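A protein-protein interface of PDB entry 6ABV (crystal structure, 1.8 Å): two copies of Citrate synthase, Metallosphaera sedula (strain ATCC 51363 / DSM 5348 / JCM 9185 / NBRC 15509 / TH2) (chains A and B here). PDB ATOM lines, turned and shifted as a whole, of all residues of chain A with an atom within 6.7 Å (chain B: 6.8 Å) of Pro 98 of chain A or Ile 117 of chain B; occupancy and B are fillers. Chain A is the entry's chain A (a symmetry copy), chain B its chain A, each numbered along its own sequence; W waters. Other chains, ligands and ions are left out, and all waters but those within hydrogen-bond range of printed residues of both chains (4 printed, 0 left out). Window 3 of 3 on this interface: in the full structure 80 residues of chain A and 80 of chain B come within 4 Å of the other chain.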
ATOM      1  N   ILE A  94     -14.890 -28.485  -5.175  1.00  0.00           N
ATOM      2  CA  ILE A  94     -15.796 -29.528  -4.794  1.00  0.00           C
ATOM      3  C   ILE A  94     -15.988 -29.517  -3.265  1.00  0.00           C
ATOM      4  O   ILE A  94     -17.079 -29.604  -2.681  1.00  0.00           O
ATOM      5  CB  ILE A  94     -15.219 -30.888  -5.295  1.00  0.00           C
ATOM      6  CG1 ILE A  94     -15.327 -30.966  -6.820  1.00  0.00           C
ATOM      7  CG2 ILE A  94     -16.084 -32.046  -4.760  1.00  0.00           C
ATOM      8  CD1 ILE A  94     -14.674 -32.214  -7.472  1.00  0.00           C
ATOM      9  N   TYR A  95     -14.849 -29.502  -2.644  1.00  0.00           N
ATOM     10  CA  TYR A  95     -14.798 -29.512  -1.176  1.00  0.00           C
ATOM     11  C   TYR A  95     -15.217 -28.199  -0.495  1.00  0.00           C
ATOM     12  O   TYR A  95     -15.488 -28.224   0.705  1.00  0.00           O
ATOM     13  CB  TYR A  95     -13.369 -29.897  -0.723  1.00  0.00           C
ATOM     14  CG  TYR A  95     -13.179 -31.385  -0.685  1.00  0.00           C
ATOM     15  CD1 TYR A  95     -12.805 -32.073  -1.820  1.00  0.00           C
ATOM     16  CD2 TYR A  95     -13.335 -32.107   0.499  1.00  0.00           C
ATOM     17  CE1 TYR A  95     -12.615 -33.465  -1.815  1.00  0.00           C
ATOM     18  CE2 TYR A  95     -13.112 -33.466   0.529  1.00  0.00           C
ATOM     19  CZ  TYR A  95     -12.749 -34.149  -0.602  1.00  0.00           C
ATOM     20  OH  TYR A  95     -12.597 -35.509  -0.589  1.00  0.00           O
ATOM     21  N   SER A  96     -15.293 -27.071  -1.236  1.00  0.00           N
ATOM     22  CA  SER A  96     -15.848 -25.822  -0.661  1.00  0.00           C
ATOM     23  C   SER A  96     -17.417 -25.708  -0.764  1.00  0.00           C
ATOM     24  O   SER A  96     -18.029 -24.890  -0.090  1.00  0.00           O
ATOM     25  CB  SER A  96     -15.153 -24.644  -1.329  1.00  0.00           C
ATOM     26  OG  SER A  96     -15.654 -24.542  -2.651  1.00  0.00           O
ATOM     27  N   LEU A  97     -18.084 -26.528  -1.583  1.00  0.00           N
ATOM     28  CA  LEU A  97     -19.509 -26.515  -1.614  1.00  0.00           C
ATOM     29  C   LEU A  97     -20.164 -27.094  -0.359  1.00  0.00           C
ATOM     30  O   LEU A  97     -19.577 -27.960   0.304  1.00  0.00           O
ATOM     31  CB  LEU A  97     -20.040 -27.181  -2.884  1.00  0.00           C
ATOM     32  CG  LEU A  97     -19.662 -26.474  -4.159  1.00  0.00           C
ATOM     33  CD1 LEU A  97     -20.024 -27.460  -5.323  1.00  0.00           C
ATOM     34  CD2 LEU A  97     -20.359 -25.149  -4.209  1.00  0.00           C
ATOM     35  N   PRO A  98     -21.379 -26.648  -0.032  1.00  0.00           N
ATOM     36  CA  PRO A  98     -22.036 -27.367   1.087  1.00  0.00           C
ATOM     37  C   PRO A  98     -22.116 -28.885   0.901  1.00  0.00           C
ATOM     38  O   PRO A  98     -22.450 -29.364  -0.179  1.00  0.00           O
ATOM     39  CB  PRO A  98     -23.421 -26.788   1.110  1.00  0.00           C
ATOM     40  CG  PRO A  98     -23.277 -25.435   0.511  1.00  0.00           C
ATOM     41  CD  PRO A  98     -22.209 -25.558  -0.553  1.00  0.00           C
ATOM     42  N   ARG A  99     -21.753 -29.650   1.930  1.00  0.00           N
ATOM     43  CA  ARG A  99     -21.735 -31.109   1.800  1.00  0.00           C
ATOM     44  C   ARG A  99     -23.073 -31.760   1.492  1.00  0.00           C
ATOM     45  O   ARG A  99     -23.114 -32.960   1.093  1.00  0.00           O
ATOM     46  CB  ARG A  99     -21.164 -31.742   3.098  1.00  0.00           C
ATOM     47  CG  ARG A  99     -19.679 -31.491   3.262  1.00  0.00           C
ATOM     48  CD  ARG A  99     -19.138 -32.093   4.569  1.00  0.00           C
ATOM     49  NE  ARG A  99     -19.592 -33.458   4.676  1.00  0.00           N
ATOM     50  CZ  ARG A  99     -19.650 -34.200   5.786  1.00  0.00           C
ATOM     51  NH1 ARG A  99     -19.256 -33.719   6.965  1.00  0.00           N
ATOM     52  NH2 ARG A  99     -20.106 -35.451   5.698  1.00  0.00           N
ATOM     53  N   ASP A 100     -24.166 -31.040   1.744  1.00  0.00           N
ATOM     54  CA  ASP A 100     -25.517 -31.520   1.431  1.00  0.00           C
ATOM     55  C   ASP A 100     -25.974 -31.087   0.046  1.00  0.00           C
ATOM     56  O   ASP A 100     -27.101 -31.317  -0.302  1.00  0.00           O
ATOM     57  CB  ASP A 100     -26.520 -31.166   2.533  1.00  0.00           C
ATOM     58  CG  ASP A 100     -26.815 -29.684   2.630  1.00  0.00           C
ATOM     59  OD1 ASP A 100     -25.979 -28.864   2.194  1.00  0.00           O
ATOM     60  OD2 ASP A 100     -27.899 -29.357   3.161  1.00  0.00           O
ATOM     61  N   SER A 101     -25.085 -30.485  -0.734  1.00  0.00           N
ATOM     62  CA  SER A 101     -25.426 -30.059  -2.121  1.00  0.00           C
ATOM     63  C   SER A 101     -25.641 -31.306  -3.009  1.00  0.00           C
ATOM     64  O   SER A 101     -24.952 -32.330  -2.829  1.00  0.00           O
ATOM     65  CB  SER A 101     -24.285 -29.265  -2.728  1.00  0.00           C
ATOM     66  OG  SER A 101     -24.021 -28.066  -2.070  1.00  0.00           O
ATOM     67  N   ASP A 102     -26.535 -31.167  -3.961  1.00  0.00           N
ATOM     68  CA  ASP A 102     -26.815 -32.209  -4.940  1.00  0.00           C
ATOM     69  C   ASP A 102     -25.513 -32.594  -5.645  1.00  0.00           C
ATOM     70  O   ASP A 102     -24.741 -31.726  -6.107  1.00  0.00           O
ATOM     71  CB  ASP A 102     -27.872 -31.779  -5.874  1.00  0.00           C
ATOM     72  CG  ASP A 102     -28.343 -32.937  -6.729  1.00  0.00           C
ATOM     73  OD1 ASP A 102     -27.675 -33.173  -7.701  1.00  0.00           O
ATOM     74  OD2 ASP A 102     -29.230 -33.720  -6.332  1.00  0.00           O
ATOM     75  N   MET A 106     -22.566 -30.444  -7.817  1.00  0.00           N
ATOM     76  CA  MET A 106     -21.163 -30.464  -7.544  1.00  0.00           C
ATOM     77  C   MET A 106     -20.367 -30.847  -8.768  1.00  0.00           C
ATOM     78  O   MET A 106     -19.373 -30.241  -9.075  1.00  0.00           O
ATOM     79  CB  MET A 106     -20.854 -31.366  -6.337  1.00  0.00           C
ATOM     80  CG  MET A 106     -21.561 -30.849  -5.125  1.00  0.00           C
ATOM     81  SD  MET A 106     -21.336 -31.994  -3.701  1.00  0.00           S
ATOM     82  CE  MET A 106     -19.664 -31.830  -3.442  1.00  0.00           C
ATOM     83  N   LYS A 149     -18.687 -35.233   0.050  1.00  0.00           N
ATOM     84  CA  LYS A 149     -19.935 -35.309   0.719  1.00  0.00           C
ATOM     85  C   LYS A 149     -19.810 -36.236   1.954  1.00  0.00           C
ATOM     86  O   LYS A 149     -20.595 -36.067   2.907  1.00  0.00           O
ATOM     87  CB  LYS A 149     -21.063 -35.826  -0.168  1.00  0.00           C
ATOM     88  CG  LYS A 149     -21.476 -34.825  -1.256  1.00  0.00           C
ATOM     89  CD  LYS A 149     -22.558 -35.269  -2.195  1.00  0.00           C
ATOM     90  CE  LYS A 149     -23.922 -35.459  -1.557  1.00  0.00           C
ATOM     91  NZ  LYS A 149     -24.483 -34.229  -0.979  1.00  0.00           N
ATOM     92  N   LYS A 225     -29.600 -32.084 -13.609  1.00  0.00           N
ATOM     93  CA  LYS A 225     -29.930 -31.755 -12.259  1.00  0.00           C
ATOM     94  C   LYS A 225     -31.427 -31.599 -12.058  1.00  0.00           C
ATOM     95  O   LYS A 225     -31.887 -31.739 -10.900  1.00  0.00           O
ATOM     96  CB  LYS A 225     -29.226 -30.436 -11.837  1.00  0.00           C
ATOM     97  CG  LYS A 225     -29.167 -30.160 -10.368  1.00  0.00           C
ATOM     98  CD  LYS A 225     -28.647 -28.710 -10.177  1.00  0.00           C
ATOM     99  CE  LYS A 225     -28.675 -28.463  -8.707  1.00  0.00           C
ATOM    100  NZ  LYS A 225     -28.354 -27.049  -8.427  1.00  0.00           N
ATOM    101  N   PRO B  87     -22.008 -16.326  -0.628  1.00  0.00           N
ATOM    102  CA  PRO B  87     -20.990 -16.863   0.310  1.00  0.00           C
ATOM    103  C   PRO B  87     -19.623 -16.704  -0.178  1.00  0.00           C
ATOM    104  O   PRO B  87     -19.351 -16.741  -1.370  1.00  0.00           O
ATOM    105  CB  PRO B  87     -21.356 -18.347   0.437  1.00  0.00           C
ATOM    106  CG  PRO B  87     -22.785 -18.430  -0.008  1.00  0.00           C
ATOM    107  CD  PRO B  87     -22.913 -17.377  -1.098  1.00  0.00           C
ATOM    108  N   GLN B  89     -17.325 -18.686  -0.332  1.00  0.00           N
ATOM    109  CA  GLN B  89     -16.848 -19.778  -1.198  1.00  0.00           C
ATOM    110  C   GLN B  89     -17.028 -19.463  -2.660  1.00  0.00           C
ATOM    111  O   GLN B  89     -16.232 -19.877  -3.437  1.00  0.00           O
ATOM    112  CB  GLN B  89     -17.521 -21.113  -0.852  1.00  0.00           C
ATOM    113  CG  GLN B  89     -17.080 -21.602   0.542  1.00  0.00           C
ATOM    114  CD  GLN B  89     -17.997 -21.150   1.707  1.00  0.00           C
ATOM    115  OE1 GLN B  89     -18.580 -20.062   1.719  1.00  0.00           O
ATOM    116  NE2 GLN B  89     -18.148 -22.037   2.696  1.00  0.00           N
ATOM    117  N   VAL B  90     -18.080 -18.726  -3.004  1.00  0.00           N
ATOM    118  CA  VAL B  90     -18.319 -18.369  -4.405  1.00  0.00           C
ATOM    119  C   VAL B  90     -17.225 -17.411  -4.930  1.00  0.00           C
ATOM    120  O   VAL B  90     -16.677 -17.604  -6.003  1.00  0.00           O
ATOM    121  CB  VAL B  90     -19.707 -17.796  -4.604  1.00  0.00           C
ATOM    122  CG1 VAL B  90     -19.897 -17.276  -6.024  1.00  0.00           C
ATOM    123  CG2 VAL B  90     -20.748 -18.840  -4.285  1.00  0.00           C
ATOM    124  N   MET B  93     -13.868 -19.249  -5.371  1.00  0.00           N
ATOM    125  CA  MET B  93     -13.797 -20.005  -6.630  1.00  0.00           C
ATOM    126  C   MET B  93     -13.379 -19.223  -7.816  1.00  0.00           C
ATOM    127  O   MET B  93     -12.560 -19.684  -8.604  1.00  0.00           O
ATOM    128  CB  MET B  93     -15.099 -20.719  -6.875  1.00  0.00           C
ATOM    129  CG  MET B  93     -15.400 -21.689  -5.733  1.00  0.00           C
ATOM    130  SD  MET B  93     -16.993 -22.573  -5.767  1.00  0.00           S
ATOM    131  CE  MET B  93     -16.739 -23.032  -7.383  1.00  0.00           C
ATOM    132  N   SER B 112     -22.506 -21.918 -11.331  1.00  0.00           N
ATOM    133  CA  SER B 112     -22.649 -23.304 -10.902  1.00  0.00           C
ATOM    134  C   SER B 112     -22.662 -23.442  -9.389  1.00  0.00           C
ATOM    135  O   SER B 112     -23.538 -24.126  -8.803  1.00  0.00           O
ATOM    136  CB  SER B 112     -21.613 -24.297 -11.601  1.00  0.00           C
ATOM    137  OG  SER B 112     -21.676 -24.249 -13.035  1.00  0.00           O
ATOM    138  N   ALA B 113     -21.717 -22.757  -8.771  1.00  0.00           N
ATOM    139  CA  ALA B 113     -21.656 -22.735  -7.311  1.00  0.00           C
ATOM    140  C   ALA B 113     -22.876 -22.085  -6.686  1.00  0.00           C
ATOM    141  O   ALA B 113     -23.452 -22.608  -5.750  1.00  0.00           O
ATOM    142  CB  ALA B 113     -20.349 -22.035  -6.956  1.00  0.00           C
ATOM    143  N   LEU B 114     -23.349 -20.961  -7.243  1.00  0.00           N
ATOM    144  CA  LEU B 114     -24.638 -20.352  -6.855  1.00  0.00           C
ATOM    145  C   LEU B 114     -25.818 -21.281  -7.015  1.00  0.00           C
ATOM    146  O   LEU B 114     -26.660 -21.339  -6.166  1.00  0.00           O
ATOM    147  CB  LEU B 114     -24.886 -19.021  -7.615  1.00  0.00           C
ATOM    148  CG  LEU B 114     -23.944 -17.883  -7.384  1.00  0.00           C
ATOM    149  CD1 LEU B 114     -24.097 -16.700  -8.354  1.00  0.00           C
ATOM    150  CD2 LEU B 114     -24.096 -17.464  -5.956  1.00  0.00           C
ATOM    151  N   SER B 115     -25.888 -22.056  -8.119  1.00  0.00           N
ATOM    152  CA  SER B 115     -26.895 -23.046  -8.250  1.00  0.00           C
ATOM    153  C   SER B 115     -26.900 -24.119  -7.121  1.00  0.00           C
ATOM    154  O   SER B 115     -27.943 -24.459  -6.590  1.00  0.00           O
ATOM    155  CB  SER B 115     -26.743 -23.746  -9.615  1.00  0.00           C
ATOM    156  OG  SER B 115     -27.835 -24.592  -9.873  1.00  0.00           O
ATOM    157  N   SER B 116     -25.717 -24.595  -6.782  1.00  0.00           N
ATOM    158  CA  SER B 116     -25.567 -25.616  -5.729  1.00  0.00           C
ATOM    159  C   SER B 116     -25.974 -25.025  -4.381  1.00  0.00           C
ATOM    160  O   SER B 116     -26.523 -25.754  -3.545  1.00  0.00           O
ATOM    161  CB  SER B 116     -24.083 -26.077  -5.684  1.00  0.00           C
ATOM    162  OG  SER B 116     -23.778 -26.835  -6.875  1.00  0.00           O
ATOM    163  N   ILE B 117     -25.646 -23.742  -4.144  1.00  0.00           N
ATOM    164  CA  ILE B 117     -25.963 -23.101  -2.823  1.00  0.00           C
ATOM    165  C   ILE B 117     -27.446 -22.637  -2.713  1.00  0.00           C
ATOM    166  O   ILE B 117     -28.151 -22.866  -1.699  1.00  0.00           O
ATOM    167  CB  ILE B 117     -24.958 -21.954  -2.597  1.00  0.00           C
ATOM    168  CG1 ILE B 117     -23.577 -22.540  -2.377  1.00  0.00           C
ATOM    169  CG2 ILE B 117     -25.428 -21.042  -1.456  1.00  0.00           C
ATOM    170  CD1 ILE B 117     -22.440 -21.603  -2.640  1.00  0.00           C
ATOM    171  N   TYR B 118     -27.938 -21.974  -3.763  1.00  0.00           N
ATOM    172  CA  TYR B 118     -29.215 -21.285  -3.734  1.00  0.00           C
ATOM    173  C   TYR B 118     -30.304 -21.892  -4.537  1.00  0.00           C
ATOM    174  O   TYR B 118     -31.456 -21.417  -4.448  1.00  0.00           O
ATOM    175  CB  TYR B 118     -29.068 -19.870  -4.212  1.00  0.00           C
ATOM    176  CG  TYR B 118     -28.258 -18.948  -3.353  1.00  0.00           C
ATOM    177  CD1 TYR B 118     -28.718 -18.590  -2.049  1.00  0.00           C
ATOM    178  CD2 TYR B 118     -27.025 -18.427  -3.825  1.00  0.00           C
ATOM    179  CE1 TYR B 118     -27.948 -17.700  -1.267  1.00  0.00           C
ATOM    180  CE2 TYR B 118     -26.261 -17.495  -3.051  1.00  0.00           C
ATOM    181  CZ  TYR B 118     -26.771 -17.148  -1.778  1.00  0.00           C
ATOM    182  OH  TYR B 118     -26.014 -16.259  -1.014  1.00  0.00           O
ATOM    183  N   GLY B 119     -29.980 -22.876  -5.349  1.00  0.00           N
ATOM    184  CA  GLY B 119     -30.999 -23.441  -6.326  1.00  0.00           C
ATOM    185  C   GLY B 119     -32.232 -23.940  -5.600  1.00  0.00           C
ATOM    186  O   GLY B 119     -32.101 -24.728  -4.611  1.00  0.00           O
ATOM    187  N   MET B 120     -33.410 -23.507  -6.063  1.00  0.00           N
ATOM    188  CA  MET B 120     -34.672 -23.981  -5.504  1.00  0.00           C
ATOM    189  C   MET B 120     -35.570 -24.529  -6.599  1.00  0.00           C
ATOM    190  O   MET B 120     -35.455 -24.124  -7.728  1.00  0.00           O
ATOM    191  CB  MET B 120     -35.380 -22.805  -4.763  1.00  0.00           C
ATOM    192  CG  MET B 120     -34.689 -22.391  -3.531  1.00  0.00           C
ATOM    193  SD  MET B 120     -34.830 -23.631  -2.213  1.00  0.00           S
ATOM    194  CE  MET B 120     -36.485 -23.202  -1.605  1.00  0.00           C
HETATM  195  O   HOH W   1     -25.399 -26.830  -9.185  1.00  0.00           O
HETATM  196  O   HOH W   2     -27.953 -28.551  -4.227  1.00  0.00           O
HETATM  197  O   HOH W   3     -26.741 -26.886  -0.596  1.00  0.00           O
HETATM  198  O   HOH W   4     -25.503 -29.010  -6.238  1.00  0.00           O
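The side-chain hydroxyl (OG) of Ser 115 of chain B lies within hydrogen-bond range of the side-chain amino group (NZ) of Lys 225 of chain A, at 2.9 Å.
The side-chain hydroxyl (OG) of Ser 116 of chain B is in hydrogen-bond range of the backbone carbonyl oxygen (O) of Ser 112 of chain B, at 3.3 Å.
O of Pro 98 of chain A is in hydrogen-bond range of OG of Ser 101 of chain A.
The backbone carbonyl oxygen of Ser 101 of chain A sits at hydrogen-bond distance from the side-chain amino group of Lys 149 of chain A.
Of the printed residues of chain B, Ser 96 of chain A touches Gln 89 (3.5 Å) and Met 93 (3.9 Å).
Pro 98 of chain A touches just one residue of chain B: Ile 117 (3.8 Å).
Of the printed residues of chain B, Ser 101 of chain A touches Ser 116.
Leu 114 of chain B touches none of the printed residues of chain A.
Of the printed residues of chain A, Ser 115 of chain B touches Lys 225 (2.9 Å).
Ile 117 of chain B touches one residue of chain A.
The nearest residue of chain B that does not touch Pro 98 of chain A is Ser 116 of chain B (5.2 Å).
Along chain B the printed residues that touch a printed residue of chain A span positions 89 to 117.
Among the printed residues, no Asp or Glu carboxylate lies within 4 Å of a Lys or Arg side-chain nitrogen of the other chain.
Among the printed residues, merely in contact across the chains: Ser 96 of chain A with Gln 89 of chain B (3.5 Å), Ser 101 of chain A with Ser 116 of chain B (3.7 Å), Pro 98 of chain A with Ile 117 of chain B (3.8 Å), Ser 96 of chain A with Met 93 of chain B (3.9 Å), Met 106 of chain A with Ser 116 of chain B (3.9 Å) and Lys 225 of chain A with Ser 116 of chain B (3.96 Å).
Water W1 lies within hydrogen-bond range of the side-chain hydroxyl (OG) of Ser 116 of chain B (2.8 Å), the side-chain amino group (NZ) of Lys 225 of chain A (3.1 Å), the backbone carbonyl oxygen (O) of Ser 112 of chain B (3.3 Å) and the side-chain hydroxyl (OG) of Ser 115 of chain B (3.4 Å).
Water W4 bridges the backbone carbonyl oxygen of Asp 102 of chain A (2.8 Å) and the side-chain hydroxyl of Ser 116 of chain B (2.8 Å).
Water W2 bridges the backbone NH of Asp 102 of chain A and the backbone carbonyl oxygen of Ser 116 of chain B.
Water W3 bridges the backbone carbonyl oxygen (O) of Ser 116 of chain B (3.2 Å) and the side-chain hydroxyl (OG) of Ser 101 of chain A (3.3 Å).
No position is printed for both chains.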
